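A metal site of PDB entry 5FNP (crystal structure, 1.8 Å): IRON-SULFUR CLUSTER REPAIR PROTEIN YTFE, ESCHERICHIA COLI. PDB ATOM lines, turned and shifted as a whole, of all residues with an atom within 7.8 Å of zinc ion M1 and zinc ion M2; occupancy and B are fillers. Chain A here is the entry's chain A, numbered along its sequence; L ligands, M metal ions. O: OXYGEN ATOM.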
ATOM      1  N   ILE A  79      19.435  11.775   5.475  1.00  0.00           N
ATOM      2  CA  ILE A  79      20.721  12.425   5.777  1.00  0.00           C
ATOM      3  C   ILE A  79      20.512  13.787   6.427  1.00  0.00           C
ATOM      4  O   ILE A  79      21.153  14.114   7.442  1.00  0.00           O
ATOM      5  CB  ILE A  79      21.576  12.538   4.530  1.00  0.00           C
ATOM      6  CG1 ILE A  79      22.073  11.136   4.134  1.00  0.00           C
ATOM      7  CG2 ILE A  79      22.777  13.435   4.773  1.00  0.00           C
ATOM      8  CD1 ILE A  79      22.659  11.098   2.739  1.00  0.00           C
ATOM      9  N   ILE A  80      19.676  14.605   5.815  1.00  0.00           N
ATOM     10  CA  ILE A  80      19.489  15.981   6.288  1.00  0.00           C
ATOM     11  C   ILE A  80      19.044  15.971   7.743  1.00  0.00           C
ATOM     12  O   ILE A  80      19.590  16.728   8.586  1.00  0.00           O
ATOM     13  CB  ILE A  80      18.497  16.772   5.402  1.00  0.00           C
ATOM     14  CG1 ILE A  80      19.117  17.058   4.038  1.00  0.00           C
ATOM     15  CG2 ILE A  80      18.090  18.093   6.063  1.00  0.00           C
ATOM     16  CD1 ILE A  80      18.112  17.422   2.966  1.00  0.00           C
ATOM     17  N   TYR A  83      21.396  13.197  10.205  1.00  0.00           N
ATOM     18  CA  TYR A  83      22.793  13.542  10.330  1.00  0.00           C
ATOM     19  C   TYR A  83      23.091  15.057  10.296  1.00  0.00           C
ATOM     20  O   TYR A  83      23.632  15.575  11.266  1.00  0.00           O
ATOM     21  CB  TYR A  83      23.636  12.746   9.310  1.00  0.00           C
ATOM     22  CG  TYR A  83      23.543  11.256   9.540  1.00  0.00           C
ATOM     23  CD1 TYR A  83      23.971  10.681  10.741  1.00  0.00           C
ATOM     24  CD2 TYR A  83      23.049  10.417   8.560  1.00  0.00           C
ATOM     25  CE1 TYR A  83      23.842   9.310  10.972  1.00  0.00           C
ATOM     26  CE2 TYR A  83      22.969   9.038   8.748  1.00  0.00           C
ATOM     27  CZ  TYR A  83      23.370   8.499   9.959  1.00  0.00           C
ATOM     28  OH  TYR A  83      23.300   7.135  10.130  1.00  0.00           O
ATOM     29  N   HIS A  84      22.752  15.762   9.209  1.00  0.00           N
ATOM     30  CA  HIS A  84      23.161  17.168   9.105  1.00  0.00           C
ATOM     31  C   HIS A  84      22.614  17.995  10.277  1.00  0.00           C
ATOM     32  O   HIS A  84      23.359  18.679  10.952  1.00  0.00           O
ATOM     33  CB  HIS A  84      22.684  17.804   7.823  1.00  0.00           C
ATOM     34  CG  HIS A  84      23.374  17.295   6.602  1.00  0.00           C
ATOM     35  ND1 HIS A  84      23.280  17.944   5.392  1.00  0.00           N
ATOM     36  CD2 HIS A  84      24.251  16.278   6.420  1.00  0.00           C
ATOM     37  CE1 HIS A  84      24.059  17.332   4.505  1.00  0.00           C
ATOM     38  NE2 HIS A  84      24.660  16.332   5.098  1.00  0.00           N
ATOM     39  N   HIS A  87      24.357  17.073  13.578  1.00  0.00           N
ATOM     40  CA  HIS A  87      25.716  17.631  13.693  1.00  0.00           C
ATOM     41  C   HIS A  87      25.650  19.118  14.070  1.00  0.00           C
ATOM     42  O   HIS A  87      26.450  19.581  14.861  1.00  0.00           O
ATOM     43  CB  HIS A  87      26.528  17.482  12.405  1.00  0.00           C
ATOM     44  CG  HIS A  87      26.724  16.066  11.933  1.00  0.00           C
ATOM     45  ND1 HIS A  87      26.812  14.990  12.787  1.00  0.00           N
ATOM     46  CD2 HIS A  87      26.929  15.565  10.694  1.00  0.00           C
ATOM     47  CE1 HIS A  87      27.017  13.889  12.100  1.00  0.00           C
ATOM     48  NE2 HIS A  87      27.073  14.196  10.827  1.00  0.00           N
ATOM     49  N   LEU A 126      32.417  21.508   8.268  1.00  0.00           N
ATOM     50  CA  LEU A 126      31.273  20.684   8.047  1.00  0.00           C
ATOM     51  C   LEU A 126      30.029  21.518   7.747  1.00  0.00           C
ATOM     52  O   LEU A 126      29.225  21.168   6.889  1.00  0.00           O
ATOM     53  CB  LEU A 126      31.047  19.756   9.219  1.00  0.00           C
ATOM     54  CG  LEU A 126      30.140  18.566   9.113  1.00  0.00           C
ATOM     55  CD1 LEU A 126      30.662  17.590   8.069  1.00  0.00           C
ATOM     56  CD2 LEU A 126      30.069  17.913  10.483  1.00  0.00           C
ATOM     57  N   HIS A 129      30.232  22.706   4.116  1.00  0.00           N
ATOM     58  CA  HIS A 129      30.051  21.500   3.299  1.00  0.00           C
ATOM     59  C   HIS A 129      28.589  21.047   3.226  1.00  0.00           C
ATOM     60  O   HIS A 129      28.064  20.806   2.138  1.00  0.00           O
ATOM     61  CB  HIS A 129      30.979  20.367   3.840  1.00  0.00           C
ATOM     62  CG  HIS A 129      30.746  19.010   3.262  1.00  0.00           C
ATOM     63  ND1 HIS A 129      31.557  18.483   2.260  1.00  0.00           N
ATOM     64  CD2 HIS A 129      29.891  18.019   3.610  1.00  0.00           C
ATOM     65  CE1 HIS A 129      31.172  17.248   2.004  1.00  0.00           C
ATOM     66  NE2 HIS A 129      30.162  16.935   2.802  1.00  0.00           N
ATOM     67  N   MET A 130      27.932  20.918   4.383  1.00  0.00           N
ATOM     68  CA  MET A 130      26.550  20.488   4.452  1.00  0.00           C
ATOM     69  C   MET A 130      25.604  21.458   3.725  1.00  0.00           C
ATOM     70  O   MET A 130      24.640  21.039   3.111  1.00  0.00           O
ATOM     71  CB  MET A 130      26.092  20.287   5.880  1.00  0.00           C
ATOM     72  CG  MET A 130      26.807  19.106   6.523  1.00  0.00           C
ATOM     73  SD  MET A 130      26.262  18.652   8.175  1.00  0.00           S
ATOM     74  CE  MET A 130      26.544  20.196   9.040  1.00  0.00           C
ATOM     75  N   MET A 131      25.886  22.753   3.828  1.00  0.00           N
ATOM     76  CA  MET A 131      25.076  23.772   3.129  1.00  0.00           C
ATOM     77  C   MET A 131      25.170  23.615   1.622  1.00  0.00           C
ATOM     78  O   MET A 131      24.188  23.730   0.919  1.00  0.00           O
ATOM     79  CB  MET A 131      25.491  25.200   3.520  1.00  0.00           C
ATOM     80  CG  MET A 131      24.636  26.314   2.897  1.00  0.00           C
ATOM     81  SD  MET A 131      25.230  27.953   3.345  1.00  0.00           S
ATOM     82  CE  MET A 131      26.420  28.221   2.040  1.00  0.00           C
ATOM     83  N   GLU A 133      25.776  20.797   0.028  1.00  0.00           N
ATOM     84  CA  GLU A 133      24.983  19.633  -0.275  1.00  0.00           C
ATOM     85  C   GLU A 133      23.495  19.947  -0.309  1.00  0.00           C
ATOM     86  O   GLU A 133      22.747  19.517  -1.200  1.00  0.00           O
ATOM     87  CB  GLU A 133      25.253  18.491   0.707  1.00  0.00           C
ATOM     88  CG  GLU A 133      26.639  17.861   0.519  1.00  0.00           C
ATOM     89  CD  GLU A 133      26.993  16.745   1.510  1.00  0.00           C
ATOM     90  OE1 GLU A 133      26.297  16.621   2.563  1.00  0.00           O
ATOM     91  OE2 GLU A 133      27.983  15.975   1.265  1.00  0.00           O
ATOM     92  N   GLU A 134      23.045  20.681   0.696  1.00  0.00           N
ATOM     93  CA  GLU A 134      21.604  20.975   0.795  1.00  0.00           C
ATOM     94  C   GLU A 134      21.108  21.938  -0.270  1.00  0.00           C
ATOM     95  O   GLU A 134      19.945  21.823  -0.700  1.00  0.00           O
ATOM     96  CB  GLU A 134      21.251  21.470   2.220  1.00  0.00           C
ATOM     97  CG  GLU A 134      21.304  20.312   3.227  1.00  0.00           C
ATOM     98  CD  GLU A 134      21.087  20.733   4.677  1.00  0.00           C
ATOM     99  OE1 GLU A 134      20.279  21.653   4.922  1.00  0.00           O
ATOM    100  OE2 GLU A 134      21.725  20.158   5.595  1.00  0.00           O
ATOM    101  N   LEU A 137      23.776  19.971  -4.404  1.00  0.00           N
ATOM    102  CA  LEU A 137      23.903  18.559  -4.773  1.00  0.00           C
ATOM    103  C   LEU A 137      22.660  17.752  -4.518  1.00  0.00           C
ATOM    104  O   LEU A 137      22.180  17.019  -5.399  1.00  0.00           O
ATOM    105  CB  LEU A 137      25.087  17.912  -4.071  1.00  0.00           C
ATOM    106  CG  LEU A 137      25.284  16.426  -4.386  1.00  0.00           C
ATOM    107  CD1 LEU A 137      25.474  16.226  -5.887  1.00  0.00           C
ATOM    108  CD2 LEU A 137      26.502  15.965  -3.624  1.00  0.00           C
ATOM    109  N   PHE A 138      22.075  17.892  -3.347  1.00  0.00           N
ATOM    110  CA  PHE A 138      20.871  17.138  -3.027  1.00  0.00           C
ATOM    111  C   PHE A 138      19.654  17.542  -3.928  1.00  0.00           C
ATOM    112  O   PHE A 138      19.005  16.657  -4.509  1.00  0.00           O
ATOM    113  CB  PHE A 138      20.549  17.233  -1.528  1.00  0.00           C
ATOM    114  CG  PHE A 138      21.543  16.529  -0.610  1.00  0.00           C
ATOM    115  CD1 PHE A 138      22.595  15.705  -1.088  1.00  0.00           C
ATOM    116  CD2 PHE A 138      21.397  16.622   0.768  1.00  0.00           C
ATOM    117  CE1 PHE A 138      23.451  15.077  -0.217  1.00  0.00           C
ATOM    118  CE2 PHE A 138      22.232  15.941   1.646  1.00  0.00           C
ATOM    119  CZ  PHE A 138      23.284  15.191   1.153  1.00  0.00           C
ATOM    120  N   MET A 156      32.936  16.973  -2.818  1.00  0.00           N
ATOM    121  CA  MET A 156      32.374  16.513  -1.534  1.00  0.00           C
ATOM    122  C   MET A 156      33.168  15.318  -1.001  1.00  0.00           C
ATOM    123  O   MET A 156      33.429  15.230   0.185  1.00  0.00           O
ATOM    124  CB  MET A 156      30.879  16.167  -1.646  1.00  0.00           C
ATOM    125  CG  MET A 156      29.935  17.348  -1.959  1.00  0.00           C
ATOM    126  SD  MET A 156      30.042  18.767  -0.835  1.00  0.00           S
ATOM    127  CE  MET A 156      31.277  19.835  -1.573  1.00  0.00           C
ATOM    128  N   GLU A 157      33.598  14.387  -1.889  1.00  0.00           N
ATOM    129  CA  GLU A 157      34.412  13.257  -1.419  1.00  0.00           C
ATOM    130  C   GLU A 157      35.786  13.660  -0.895  1.00  0.00           C
ATOM    131  O   GLU A 157      36.255  13.147   0.099  1.00  0.00           O
ATOM    132  CB  GLU A 157      34.527  12.163  -2.475  1.00  0.00           C
ATOM    133  CG  GLU A 157      33.165  11.487  -2.674  1.00  0.00           C
ATOM    134  CD  GLU A 157      33.211  10.240  -3.541  1.00  0.00           C
ATOM    135  OE1 GLU A 157      34.216  10.009  -4.213  1.00  0.00           O
ATOM    136  OE2 GLU A 157      32.217   9.496  -3.561  1.00  0.00           O
ATOM    137  N   GLU A 159      36.363  16.528   0.482  1.00  0.00           N
ATOM    138  CA  GLU A 159      36.071  17.131   1.788  1.00  0.00           C
ATOM    139  C   GLU A 159      35.732  16.089   2.851  1.00  0.00           C
ATOM    140  O   GLU A 159      36.096  16.249   4.016  1.00  0.00           O
ATOM    141  CB  GLU A 159      34.954  18.200   1.663  1.00  0.00           C
ATOM    142  CG  GLU A 159      35.461  19.421   0.885  1.00  0.00           C
ATOM    143  CD  GLU A 159      34.414  20.501   0.624  1.00  0.00           C
ATOM    144  OE1 GLU A 159      33.233  20.341   0.944  1.00  0.00           O
ATOM    145  OE2 GLU A 159      34.794  21.490  -0.010  1.00  0.00           O
ATOM    146  N   HIS A 160      35.106  15.005   2.478  1.00  0.00           N
ATOM    147  CA  HIS A 160      34.930  13.919   3.423  1.00  0.00           C
ATOM    148  C   HIS A 160      36.255  13.383   3.922  1.00  0.00           C
ATOM    149  O   HIS A 160      36.379  13.066   5.118  1.00  0.00           O
ATOM    150  CB  HIS A 160      34.153  12.748   2.826  1.00  0.00           C
ATOM    151  CG  HIS A 160      32.717  13.080   2.548  1.00  0.00           C
ATOM    152  ND1 HIS A 160      31.925  12.291   1.759  1.00  0.00           N
ATOM    153  CD2 HIS A 160      31.952  14.119   2.947  1.00  0.00           C
ATOM    154  CE1 HIS A 160      30.704  12.820   1.692  1.00  0.00           C
ATOM    155  NE2 HIS A 160      30.717  13.942   2.376  1.00  0.00           N
ATOM    156  N   LEU A 201      28.995  10.673  12.128  1.00  0.00           N
ATOM    157  CA  LEU A 201      29.699  11.228  10.957  1.00  0.00           C
ATOM    158  C   LEU A 201      30.221  10.120  10.026  1.00  0.00           C
ATOM    159  O   LEU A 201      30.118  10.212   8.789  1.00  0.00           O
ATOM    160  CB  LEU A 201      30.795  12.207  11.428  1.00  0.00           C
ATOM    161  CG  LEU A 201      31.428  13.162  10.433  1.00  0.00           C
ATOM    162  CD1 LEU A 201      30.463  13.823   9.491  1.00  0.00           C
ATOM    163  CD2 LEU A 201      32.276  14.205  11.207  1.00  0.00           C
ATOM    164  N   HIS A 204      27.090   8.689   8.275  1.00  0.00           N
ATOM    165  CA  HIS A 204      26.670   9.730   7.326  1.00  0.00           C
ATOM    166  C   HIS A 204      27.563   9.695   6.074  1.00  0.00           C
ATOM    167  O   HIS A 204      27.075   9.628   4.949  1.00  0.00           O
ATOM    168  CB  HIS A 204      26.779  11.062   8.084  1.00  0.00           C
ATOM    169  CG  HIS A 204      26.678  12.333   7.274  1.00  0.00           C
ATOM    170  ND1 HIS A 204      27.054  13.522   7.837  1.00  0.00           N
ATOM    171  CD2 HIS A 204      26.286  12.625   6.016  1.00  0.00           C
ATOM    172  CE1 HIS A 204      26.892  14.499   6.982  1.00  0.00           C
ATOM    173  NE2 HIS A 204      26.411  13.993   5.858  1.00  0.00           N
ATOM    174  N   ILE A 205      28.876   9.759   6.299  1.00  0.00           N
ATOM    175  CA  ILE A 205      29.814   9.750   5.151  1.00  0.00           C
ATOM    176  C   ILE A 205      29.707   8.439   4.383  1.00  0.00           C
ATOM    177  O   ILE A 205      29.759   8.474   3.150  1.00  0.00           O
ATOM    178  CB  ILE A 205      31.232  10.085   5.569  1.00  0.00           C
ATOM    179  CG1 ILE A 205      31.290  11.594   5.942  1.00  0.00           C
ATOM    180  CG2 ILE A 205      32.248   9.817   4.424  1.00  0.00           C
ATOM    181  CD1 ILE A 205      32.524  11.966   6.679  1.00  0.00           C
ATOM    182  N   GLU A 208      26.708   8.565   2.115  1.00  0.00           N
ATOM    183  CA  GLU A 208      26.976   9.396   0.940  1.00  0.00           C
ATOM    184  C   GLU A 208      27.957   8.718  -0.045  1.00  0.00           C
ATOM    185  O   GLU A 208      27.650   8.525  -1.226  1.00  0.00           O
ATOM    186  CB  GLU A 208      27.480  10.765   1.363  1.00  0.00           C
ATOM    187  CG  GLU A 208      26.329  11.580   1.950  1.00  0.00           C
ATOM    188  CD  GLU A 208      26.693  12.939   2.530  1.00  0.00           C
ATOM    189  OE1 GLU A 208      27.857  13.363   2.489  1.00  0.00           O
ATOM    190  OE2 GLU A 208      25.755  13.596   3.083  1.00  0.00           O
ATOM    191  N   ASN A 209      29.126   8.371   0.455  1.00  0.00           N
ATOM    192  CA  ASN A 209      30.180   7.821  -0.404  1.00  0.00           C
ATOM    193  C   ASN A 209      29.821   6.446  -1.001  1.00  0.00           C
ATOM    194  O   ASN A 209      30.169   6.178  -2.159  1.00  0.00           O
ATOM    195  CB  ASN A 209      31.475   7.619   0.378  1.00  0.00           C
ATOM    196  CG  ASN A 209      32.290   8.902   0.540  1.00  0.00           C
ATOM    197  OD1 ASN A 209      31.835   9.978   0.338  1.00  0.00           O
ATOM    198  ND2 ASN A 209      33.554   8.730   0.861  1.00  0.00           N
ATOM    199  N   LEU A 212      24.640   6.939  -1.829  1.00  0.00           N
ATOM    200  CA  LEU A 212      24.030   8.054  -2.557  1.00  0.00           C
ATOM    201  C   LEU A 212      24.805   8.504  -3.784  1.00  0.00           C
ATOM    202  O   LEU A 212      24.212   8.626  -4.880  1.00  0.00           O
ATOM    203  CB  LEU A 212      23.783   9.241  -1.633  1.00  0.00           C
ATOM    204  CG  LEU A 212      23.100  10.465  -2.266  1.00  0.00           C
ATOM    205  CD1 LEU A 212      21.703  10.143  -2.743  1.00  0.00           C
ATOM    206  CD2 LEU A 212      23.071  11.631  -1.279  1.00  0.00           C
ATOM    207  N   PHE A 213      26.082   8.777  -3.606  1.00  0.00           N
ATOM    208  CA  PHE A 213      26.906   9.334  -4.673  1.00  0.00           C
ATOM    209  C   PHE A 213      27.055   8.380  -5.863  1.00  0.00           C
ATOM    210  O   PHE A 213      26.776   8.802  -6.986  1.00  0.00           O
ATOM    211  CB  PHE A 213      28.269   9.798  -4.146  1.00  0.00           C
ATOM    212  CG  PHE A 213      28.211  10.981  -3.162  1.00  0.00           C
ATOM    213  CD1 PHE A 213      27.039  11.691  -2.907  1.00  0.00           C
ATOM    214  CD2 PHE A 213      29.387  11.401  -2.549  1.00  0.00           C
ATOM    215  CE1 PHE A 213      27.048  12.767  -2.025  1.00  0.00           C
ATOM    216  CE2 PHE A 213      29.398  12.499  -1.677  1.00  0.00           C
ATOM    217  CZ  PHE A 213      28.225  13.177  -1.413  1.00  0.00           C
HETATM  218  O     O L   1      28.148  15.621   4.488  1.00  0.00           O
HETATM  219 ZN    ZN M   1      26.233  15.189   4.176  1.00  0.00          ZN
HETATM  220 ZN    ZN M   2      29.020  15.229   2.720  1.00  0.00          ZN
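Zinc ion M1 is bound by an oxygen (O) of the ligand (2.0 Å), the side-chain carboxylate (OE2) of Glu 208 (2.0 Å), a ring nitrogen (NE2) of His 204 (2.1 Å), a ring nitrogen (NE2) of His 84 (2.2 Å) and the side-chain carboxylate (OE1) of Glu 133 (2.2 Å).
Zinc ion M1 has five donor atoms within binding distance.
Merely in contact with zinc ion M1: Ile 79 (3.9 Å).
Of the 24 residues printed, 5 come within 4 Å of zinc ion M1.
The nearest printed residue that does not touch zinc ion M1 is Phe 138 (4.2 Å).
OE2 of Glu 133 binds zinc ion M2.
An oxygen (O) of the ligand is bound to zinc ion M2, 2.0 Å away.
Zinc ion M2 is bound by a ring nitrogen (NE2) of His 129, at 2.1 Å.
Zinc ion M2 is bound by NE2 of His 160 (2.2 Å).
OE1 of Glu 208 binds zinc ion M2 (2.2 Å).
A ring nitrogen (ND1) of His 84 sits at hydrogen-bond distance from the side-chain carboxylate (OE2) of Glu 134, 2.7 Å away.
O of Glu 133 is in hydrogen-bond range of N of Phe 138, at 2.8 Å.
A ring nitrogen (ND1) of His 204 is in hydrogen-bond range of a ring nitrogen (NE2) of His 87.
O of Glu 208 is in hydrogen-bond range of N of Phe 213 (2.9 Å).
The backbone NH (N) of His 84 sits at hydrogen-bond distance from the backbone carbonyl oxygen (O) of Ile 79 (2.9 Å).
ND1 of His 129 is in hydrogen-bond range of OE1 of Glu 159 (2.8 Å).
ND1 of His 129 lies close to SD of Met 156, at 3.5 Å.
A ring nitrogen (ND1) of His 160 sits at hydrogen-bond distance from the side-chain amide oxygen (OD1) of Asn 209 (2.7 Å).
The nearest printed residue that does not touch zinc ion M2 is His 204 (4.3 Å).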
